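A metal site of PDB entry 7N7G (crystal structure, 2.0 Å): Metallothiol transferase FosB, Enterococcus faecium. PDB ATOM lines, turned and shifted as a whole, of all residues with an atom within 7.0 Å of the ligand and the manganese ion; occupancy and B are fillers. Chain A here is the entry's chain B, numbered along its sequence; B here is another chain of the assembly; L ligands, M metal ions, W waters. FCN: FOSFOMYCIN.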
ATOM      1  N   TYR A  64       7.297  27.465   2.332  1.00  0.00           N
ATOM      2  CA  TYR A  64       8.715  27.514   2.769  1.00  0.00           C
ATOM      3  C   TYR A  64       9.193  26.161   3.343  1.00  0.00           C
ATOM      4  O   TYR A  64      10.385  26.071   3.758  1.00  0.00           O
ATOM      5  CB  TYR A  64       8.866  28.621   3.798  1.00  0.00           C
ATOM      6  CG  TYR A  64      10.282  29.047   3.989  1.00  0.00           C
ATOM      7  CD1 TYR A  64      11.044  29.453   2.898  1.00  0.00           C
ATOM      8  CD2 TYR A  64      10.853  29.063   5.255  1.00  0.00           C
ATOM      9  CE1 TYR A  64      12.372  29.820   3.067  1.00  0.00           C
ATOM     10  CE2 TYR A  64      12.159  29.460   5.430  1.00  0.00           C
ATOM     11  CZ  TYR A  64      12.928  29.830   4.335  1.00  0.00           C
ATOM     12  OH  TYR A  64      14.214  30.208   4.502  1.00  0.00           O
ATOM     13  N   HIS A  66      10.993  22.837   3.872  1.00  0.00           N
ATOM     14  CA  HIS A  66      12.212  22.367   3.167  1.00  0.00           C
ATOM     15  C   HIS A  66      13.076  21.511   4.078  1.00  0.00           C
ATOM     16  O   HIS A  66      12.855  21.492   5.314  1.00  0.00           O
ATOM     17  CB  HIS A  66      12.979  23.577   2.576  1.00  0.00           C
ATOM     18  CG  HIS A  66      13.592  24.466   3.610  1.00  0.00           C
ATOM     19  ND1 HIS A  66      12.914  25.506   4.197  1.00  0.00           N
ATOM     20  CD2 HIS A  66      14.803  24.425   4.187  1.00  0.00           C
ATOM     21  CE1 HIS A  66      13.688  26.087   5.074  1.00  0.00           C
ATOM     22  NE2 HIS A  66      14.837  25.431   5.112  1.00  0.00           N
ATOM     23  N   ILE A  67      14.032  20.824   3.477  1.00  0.00           N
ATOM     24  CA  ILE A  67      15.052  20.018   4.187  1.00  0.00           C
ATOM     25  C   ILE A  67      16.402  20.533   3.748  1.00  0.00           C
ATOM     26  O   ILE A  67      16.597  20.711   2.542  1.00  0.00           O
ATOM     27  CB  ILE A  67      14.881  18.526   3.906  1.00  0.00           C
ATOM     28  CG1 ILE A  67      13.448  18.106   4.197  1.00  0.00           C
ATOM     29  CG2 ILE A  67      15.925  17.739   4.691  1.00  0.00           C
ATOM     30  CD1 ILE A  67      13.233  16.614   4.170  1.00  0.00           C
ATOM     31  N   ALA A  68      17.220  20.865   4.736  1.00  0.00           N
ATOM     32  CA  ALA A  68      18.584  21.415   4.606  1.00  0.00           C
ATOM     33  C   ALA A  68      19.557  20.294   4.930  1.00  0.00           C
ATOM     34  O   ALA A  68      19.380  19.598   5.950  1.00  0.00           O
ATOM     35  CB  ALA A  68      18.762  22.596   5.520  1.00  0.00           C
ATOM     36  N   ASP A 100      23.900  34.609   9.429  1.00  0.00           N
ATOM     37  CA  ASP A 100      22.915  33.565   9.070  1.00  0.00           C
ATOM     38  C   ASP A 100      23.662  32.390   8.436  1.00  0.00           C
ATOM     39  O   ASP A 100      23.061  31.314   8.277  1.00  0.00           O
ATOM     40  CB  ASP A 100      21.931  34.078   8.016  1.00  0.00           C
ATOM     41  CG  ASP A 100      20.669  34.662   8.602  1.00  0.00           C
ATOM     42  OD1 ASP A 100      20.151  34.070   9.546  1.00  0.00           O
ATOM     43  OD2 ASP A 100      20.215  35.680   8.093  1.00  0.00           O
ATOM     44  N   SER A 103      23.804  29.673   2.423  1.00  0.00           N
ATOM     45  CA  SER A 103      22.738  28.750   1.997  1.00  0.00           C
ATOM     46  C   SER A 103      22.543  28.861   0.491  1.00  0.00           C
ATOM     47  O   SER A 103      22.501  30.016  -0.040  1.00  0.00           O
ATOM     48  CB  SER A 103      21.427  29.038   2.705  1.00  0.00           C
ATOM     49  OG  SER A 103      21.529  28.689   4.078  1.00  0.00           O
ATOM     50  N   TYR A 105      19.404  27.555  -1.930  1.00  0.00           N
ATOM     51  CA  TYR A 105      18.054  26.962  -2.010  1.00  0.00           C
ATOM     52  C   TYR A 105      17.805  26.500  -3.443  1.00  0.00           C
ATOM     53  O   TYR A 105      18.169  27.226  -4.382  1.00  0.00           O
ATOM     54  CB  TYR A 105      16.980  27.947  -1.533  1.00  0.00           C
ATOM     55  CG  TYR A 105      17.190  28.375  -0.102  1.00  0.00           C
ATOM     56  CD1 TYR A 105      16.670  27.631   0.938  1.00  0.00           C
ATOM     57  CD2 TYR A 105      17.964  29.492   0.195  1.00  0.00           C
ATOM     58  CE1 TYR A 105      16.878  27.997   2.248  1.00  0.00           C
ATOM     59  CE2 TYR A 105      18.175  29.871   1.516  1.00  0.00           C
ATOM     60  CZ  TYR A 105      17.655  29.100   2.542  1.00  0.00           C
ATOM     61  OH  TYR A 105      17.858  29.443   3.845  1.00  0.00           O
ATOM     62  N   GLU A 115      17.871  22.665   0.644  1.00  0.00           N
ATOM     63  CA  GLU A 115      18.864  23.692   1.053  1.00  0.00           C
ATOM     64  C   GLU A 115      20.197  23.001   1.305  1.00  0.00           C
ATOM     65  O   GLU A 115      20.206  21.897   1.895  1.00  0.00           O
ATOM     66  CB  GLU A 115      18.358  24.440   2.276  1.00  0.00           C
ATOM     67  CG  GLU A 115      19.313  25.508   2.776  1.00  0.00           C
ATOM     68  CD  GLU A 115      18.894  26.087   4.119  1.00  0.00           C
ATOM     69  OE1 GLU A 115      17.762  25.760   4.585  1.00  0.00           O
ATOM     70  OE2 GLU A 115      19.716  26.793   4.730  1.00  0.00           O
ATOM     71  N   HIS A 117      23.437  24.122   3.397  1.00  0.00           N
ATOM     72  CA  HIS A 117      23.703  25.093   4.475  1.00  0.00           C
ATOM     73  C   HIS A 117      25.052  24.764   5.128  1.00  0.00           C
ATOM     74  O   HIS A 117      25.321  23.597   5.365  1.00  0.00           O
ATOM     75  CB  HIS A 117      22.559  25.108   5.485  1.00  0.00           C
ATOM     76  CG  HIS A 117      22.743  26.105   6.572  1.00  0.00           C
ATOM     77  ND1 HIS A 117      22.817  27.450   6.309  1.00  0.00           N
ATOM     78  CD2 HIS A 117      22.804  25.955   7.916  1.00  0.00           C
ATOM     79  CE1 HIS A 117      22.952  28.108   7.451  1.00  0.00           C
ATOM     80  NE2 HIS A 117      22.930  27.219   8.454  1.00  0.00           N
ATOM     81  N   ARG A 124      23.252  29.618  14.729  1.00  0.00           N
ATOM     82  CA  ARG A 124      21.942  30.309  14.595  1.00  0.00           C
ATOM     83  C   ARG A 124      21.449  30.780  15.976  1.00  0.00           C
ATOM     84  O   ARG A 124      21.001  31.890  16.062  1.00  0.00           O
ATOM     85  CB  ARG A 124      20.944  29.391  13.889  1.00  0.00           C
ATOM     86  CG  ARG A 124      19.647  30.080  13.503  1.00  0.00           C
ATOM     87  CD  ARG A 124      19.831  31.336  12.685  1.00  0.00           C
ATOM     88  NE  ARG A 124      20.430  31.064  11.398  1.00  0.00           N
ATOM     89  CZ  ARG A 124      19.774  30.635  10.326  1.00  0.00           C
ATOM     90  NH1 ARG A 124      18.474  30.389  10.376  1.00  0.00           N
ATOM     91  NH2 ARG A 124      20.438  30.442   9.197  1.00  0.00           N
ATOM     92  N   TYR A 128      20.860  34.758  17.098  1.00  0.00           N
ATOM     93  CA  TYR A 128      19.540  35.168  17.640  1.00  0.00           C
ATOM     94  C   TYR A 128      19.683  35.726  19.075  1.00  0.00           C
ATOM     95  O   TYR A 128      19.028  36.738  19.372  1.00  0.00           O
ATOM     96  CB  TYR A 128      18.543  34.019  17.510  1.00  0.00           C
ATOM     97  CG  TYR A 128      17.982  33.825  16.117  1.00  0.00           C
ATOM     98  CD1 TYR A 128      17.853  34.883  15.226  1.00  0.00           C
ATOM     99  CD2 TYR A 128      17.528  32.589  15.707  1.00  0.00           C
ATOM    100  CE1 TYR A 128      17.331  34.695  13.949  1.00  0.00           C
ATOM    101  CE2 TYR A 128      16.980  32.391  14.442  1.00  0.00           C
ATOM    102  CZ  TYR A 128      16.879  33.446  13.566  1.00  0.00           C
ATOM    103  OH  TYR A 128      16.354  33.227  12.322  1.00  0.00           O
ATOM    104  N   ASN B   6      21.069  18.819   7.941  1.00  0.00           N
ATOM    105  CA  ASN B   6      21.353  20.043   8.718  1.00  0.00           C
ATOM    106  C   ASN B   6      20.109  20.389   9.554  1.00  0.00           C
ATOM    107  O   ASN B   6      20.237  20.575  10.785  1.00  0.00           O
ATOM    108  CB  ASN B   6      21.759  21.205   7.812  1.00  0.00           C
ATOM    109  CG  ASN B   6      22.359  22.349   8.590  1.00  0.00           C
ATOM    110  OD1 ASN B   6      21.630  23.181   9.099  1.00  0.00           O
ATOM    111  ND2 ASN B   6      23.681  22.380   8.700  1.00  0.00           N
ATOM    112  N   HIS B   7      18.954  20.568   8.914  1.00  0.00           N
ATOM    113  CA  HIS B   7      17.690  20.868   9.632  1.00  0.00           C
ATOM    114  C   HIS B   7      16.503  20.473   8.759  1.00  0.00           C
ATOM    115  O   HIS B   7      16.722  20.213   7.541  1.00  0.00           O
ATOM    116  CB  HIS B   7      17.622  22.327  10.097  1.00  0.00           C
ATOM    117  CG  HIS B   7      17.729  23.351   9.016  1.00  0.00           C
ATOM    118  ND1 HIS B   7      18.943  23.893   8.639  1.00  0.00           N
ATOM    119  CD2 HIS B   7      16.793  23.996   8.259  1.00  0.00           C
ATOM    120  CE1 HIS B   7      18.756  24.804   7.687  1.00  0.00           C
ATOM    121  NE2 HIS B   7      17.457  24.918   7.476  1.00  0.00           N
ATOM    122  N   ILE B   8      15.344  20.359   9.409  1.00  0.00           N
ATOM    123  CA  ILE B   8      14.010  20.222   8.753  1.00  0.00           C
ATOM    124  C   ILE B   8      13.180  21.424   9.172  1.00  0.00           C
ATOM    125  O   ILE B   8      13.131  21.685  10.377  1.00  0.00           O
ATOM    126  CB  ILE B   8      13.307  18.914   9.173  1.00  0.00           C
ATOM    127  CG1 ILE B   8      14.126  17.661   8.854  1.00  0.00           C
ATOM    128  CG2 ILE B   8      11.904  18.866   8.595  1.00  0.00           C
ATOM    129  CD1 ILE B   8      13.719  16.454   9.692  1.00  0.00           C
ATOM    130  N   THR B   9      12.591  22.118   8.209  1.00  0.00           N
ATOM    131  CA  THR B   9      11.751  23.320   8.397  1.00  0.00           C
ATOM    132  C   THR B   9      10.362  23.050   7.817  1.00  0.00           C
ATOM    133  O   THR B   9      10.254  22.627   6.679  1.00  0.00           O
ATOM    134  CB  THR B   9      12.383  24.563   7.755  1.00  0.00           C
ATOM    135  OG1 THR B   9      13.587  24.830   8.491  1.00  0.00           O
ATOM    136  CG2 THR B   9      11.453  25.751   7.794  1.00  0.00           C
ATOM    137  N   LEU B  37       8.781  32.029  14.484  1.00  0.00           N
ATOM    138  CA  LEU B  37       9.569  30.761  14.379  1.00  0.00           C
ATOM    139  C   LEU B  37       9.836  30.095  15.732  1.00  0.00           C
ATOM    140  O   LEU B  37       9.701  30.714  16.790  1.00  0.00           O
ATOM    141  CB  LEU B  37      10.881  31.014  13.625  1.00  0.00           C
ATOM    142  CG  LEU B  37      11.994  31.765  14.353  1.00  0.00           C
ATOM    143  CD1 LEU B  37      12.622  30.942  15.455  1.00  0.00           C
ATOM    144  CD2 LEU B  37      13.065  32.188  13.350  1.00  0.00           C
ATOM    145  N   TYR B  39      12.529  26.659  17.199  1.00  0.00           N
ATOM    146  CA  TYR B  39      13.561  25.621  16.980  1.00  0.00           C
ATOM    147  C   TYR B  39      13.432  24.605  18.097  1.00  0.00           C
ATOM    148  O   TYR B  39      13.141  24.994  19.282  1.00  0.00           O
ATOM    149  CB  TYR B  39      14.984  26.179  16.890  1.00  0.00           C
ATOM    150  CG  TYR B  39      15.301  27.099  15.746  1.00  0.00           C
ATOM    151  CD1 TYR B  39      14.529  27.178  14.591  1.00  0.00           C
ATOM    152  CD2 TYR B  39      16.418  27.920  15.817  1.00  0.00           C
ATOM    153  CE1 TYR B  39      14.851  28.058  13.558  1.00  0.00           C
ATOM    154  CE2 TYR B  39      16.759  28.787  14.795  1.00  0.00           C
ATOM    155  CZ  TYR B  39      15.992  28.835  13.649  1.00  0.00           C
ATOM    156  OH  TYR B  39      16.364  29.717  12.666  1.00  0.00           O
ATOM    157  N   TRP B  46      17.800  19.152  14.416  1.00  0.00           N
ATOM    158  CA  TRP B  46      17.322  20.557  14.346  1.00  0.00           C
ATOM    159  C   TRP B  46      16.022  20.647  13.517  1.00  0.00           C
ATOM    160  O   TRP B  46      16.082  20.589  12.275  1.00  0.00           O
ATOM    161  CB  TRP B  46      18.421  21.415  13.742  1.00  0.00           C
ATOM    162  CG  TRP B  46      18.118  22.866  13.665  1.00  0.00           C
ATOM    163  CD1 TRP B  46      17.083  23.558  14.246  1.00  0.00           C
ATOM    164  CD2 TRP B  46      18.910  23.850  12.977  1.00  0.00           C
ATOM    165  NE1 TRP B  46      17.179  24.891  13.934  1.00  0.00           N
ATOM    166  CE2 TRP B  46      18.275  25.101  13.158  1.00  0.00           C
ATOM    167  CE3 TRP B  46      20.104  23.805  12.245  1.00  0.00           C
ATOM    168  CZ2 TRP B  46      18.799  26.291  12.626  1.00  0.00           C
ATOM    169  CZ3 TRP B  46      20.593  24.970  11.708  1.00  0.00           C
ATOM    170  CH2 TRP B  46      19.980  26.205  11.922  1.00  0.00           C
ATOM    171  N   ALA B  48      12.756  23.153  12.727  1.00  0.00           N
ATOM    172  CA  ALA B  48      12.306  24.559  12.686  1.00  0.00           C
ATOM    173  C   ALA B  48      10.857  24.630  12.189  1.00  0.00           C
ATOM    174  O   ALA B  48      10.497  23.818  11.337  1.00  0.00           O
ATOM    175  CB  ALA B  48      13.195  25.401  11.825  1.00  0.00           C
ATOM    176  N   LEU B  49      10.062  25.466  12.847  1.00  0.00           N
ATOM    177  CA  LEU B  49       8.731  25.870  12.370  1.00  0.00           C
ATOM    178  C   LEU B  49       8.827  27.356  11.993  1.00  0.00           C
ATOM    179  O   LEU B  49       9.450  28.117  12.756  1.00  0.00           O
ATOM    180  CB  LEU B  49       7.689  25.654  13.460  1.00  0.00           C
ATOM    181  CG  LEU B  49       7.682  24.289  14.136  1.00  0.00           C
ATOM    182  CD1 LEU B  49       6.718  24.324  15.290  1.00  0.00           C
ATOM    183  CD2 LEU B  49       7.329  23.183  13.166  1.00  0.00           C
ATOM    184  N   ASN B  50       8.302  27.697  10.816  1.00  0.00           N
ATOM    185  CA  ASN B  50       8.214  29.056  10.234  1.00  0.00           C
ATOM    186  C   ASN B  50       6.731  29.347   9.971  1.00  0.00           C
ATOM    187  O   ASN B  50       6.133  28.692   9.120  1.00  0.00           O
ATOM    188  CB  ASN B  50       9.039  29.161   8.957  1.00  0.00           C
ATOM    189  CG  ASN B  50      10.551  29.243   9.185  1.00  0.00           C
ATOM    190  OD1 ASN B  50      11.098  28.659  10.114  1.00  0.00           O
ATOM    191  ND2 ASN B  50      11.226  30.000   8.345  1.00  0.00           N
HETATM  192  C1  FCN L   1      14.940  28.034   7.756  1.00  0.00           C
HETATM  193  C2  FCN L   1      15.134  27.319   9.000  1.00  0.00           C
HETATM  194  C3  FCN L   1      15.966  27.939  10.072  1.00  0.00           C
HETATM  195  O   FCN L   1      15.781  26.885   7.789  1.00  0.00           O
HETATM  196  P   FCN L   1      16.027  29.215   7.060  1.00  0.00           P
HETATM  197  O1P FCN L   1      17.207  29.646   7.839  1.00  0.00           O
HETATM  198  O2P FCN L   1      15.091  30.305   6.871  1.00  0.00           O
HETATM  199  O3P FCN L   1      16.391  28.557   5.790  1.00  0.00           O
HETATM  200 MN    MN M   1      16.603  26.292   6.102  1.00  0.00          MN
HETATM  201  O   HOH W   1      14.589  30.766  10.335  1.00  0.00           O
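The manganese ion is bound by an oxygen (O) of the ligand (2.0 Å), the side-chain carboxylate of Glu 115 (2.0 Å), a ring nitrogen (NE2) of His 7 of chain B (2.1 Å), a ring nitrogen (NE2) of His 66 (2.2 Å) and an oxygen (O3P) of the ligand (2.3 Å).
OE2 of Glu 115 lies within hydrogen-bond range of OH of Tyr 105, 3.4 Å away.
The side-chain carboxylate (OE2) of Glu 115 lies within hydrogen-bond range of the side-chain hydroxyl (OG) of Ser 103 (2.7 Å).
The backbone NH (N) of Glu 115 lies within hydrogen-bond range of the backbone carbonyl oxygen (O) of Ile 67, at 3.0 Å.
O of His 7 of chain B lies within hydrogen-bond range of N of Ala 68, at 2.9 Å.
OD1 of Asn 6 of chain B is in hydrogen-bond range of ND1 of His 7 of chain B, at 2.8 Å.
O of Tyr 64 sits at hydrogen-bond distance from ND1 of His 66.
The backbone NH (N) of His 66 lies within hydrogen-bond range of the backbone carbonyl oxygen (O) of Thr 9 of chain B (2.9 Å).
NH1 of Arg 124 lies within hydrogen-bond range of OH of Tyr 39 of chain B, at 3.2 Å.
Three residues have an atom within 4 Å of the manganese ion: His 66, Glu 115 and His 7 of chain B.
The nearest printed residue that does not touch the manganese ion is Tyr 105 (4.1 Å).
An oxygen (O2P) of the ligand is in hydrogen-bond range of the side-chain hydroxyl of Tyr 64, 2.5 Å away.
O3P of the ligand lies close to OH of Tyr 105, 2.6 Å away.
NH1 of Arg 124 is in salt-bridge range of O1P of the ligand (2.9 Å).
OG1 of Thr 9 of chain B sits close to O of the ligand (3.1 Å).
Residues that only touch the ligand: Tyr 39 of chain B (3.2 Å) and Ala 48 of chain B (3.9 Å).
The nearest printed residue that does not touch the ligand is Asn 50 of chain B (4.1 Å).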
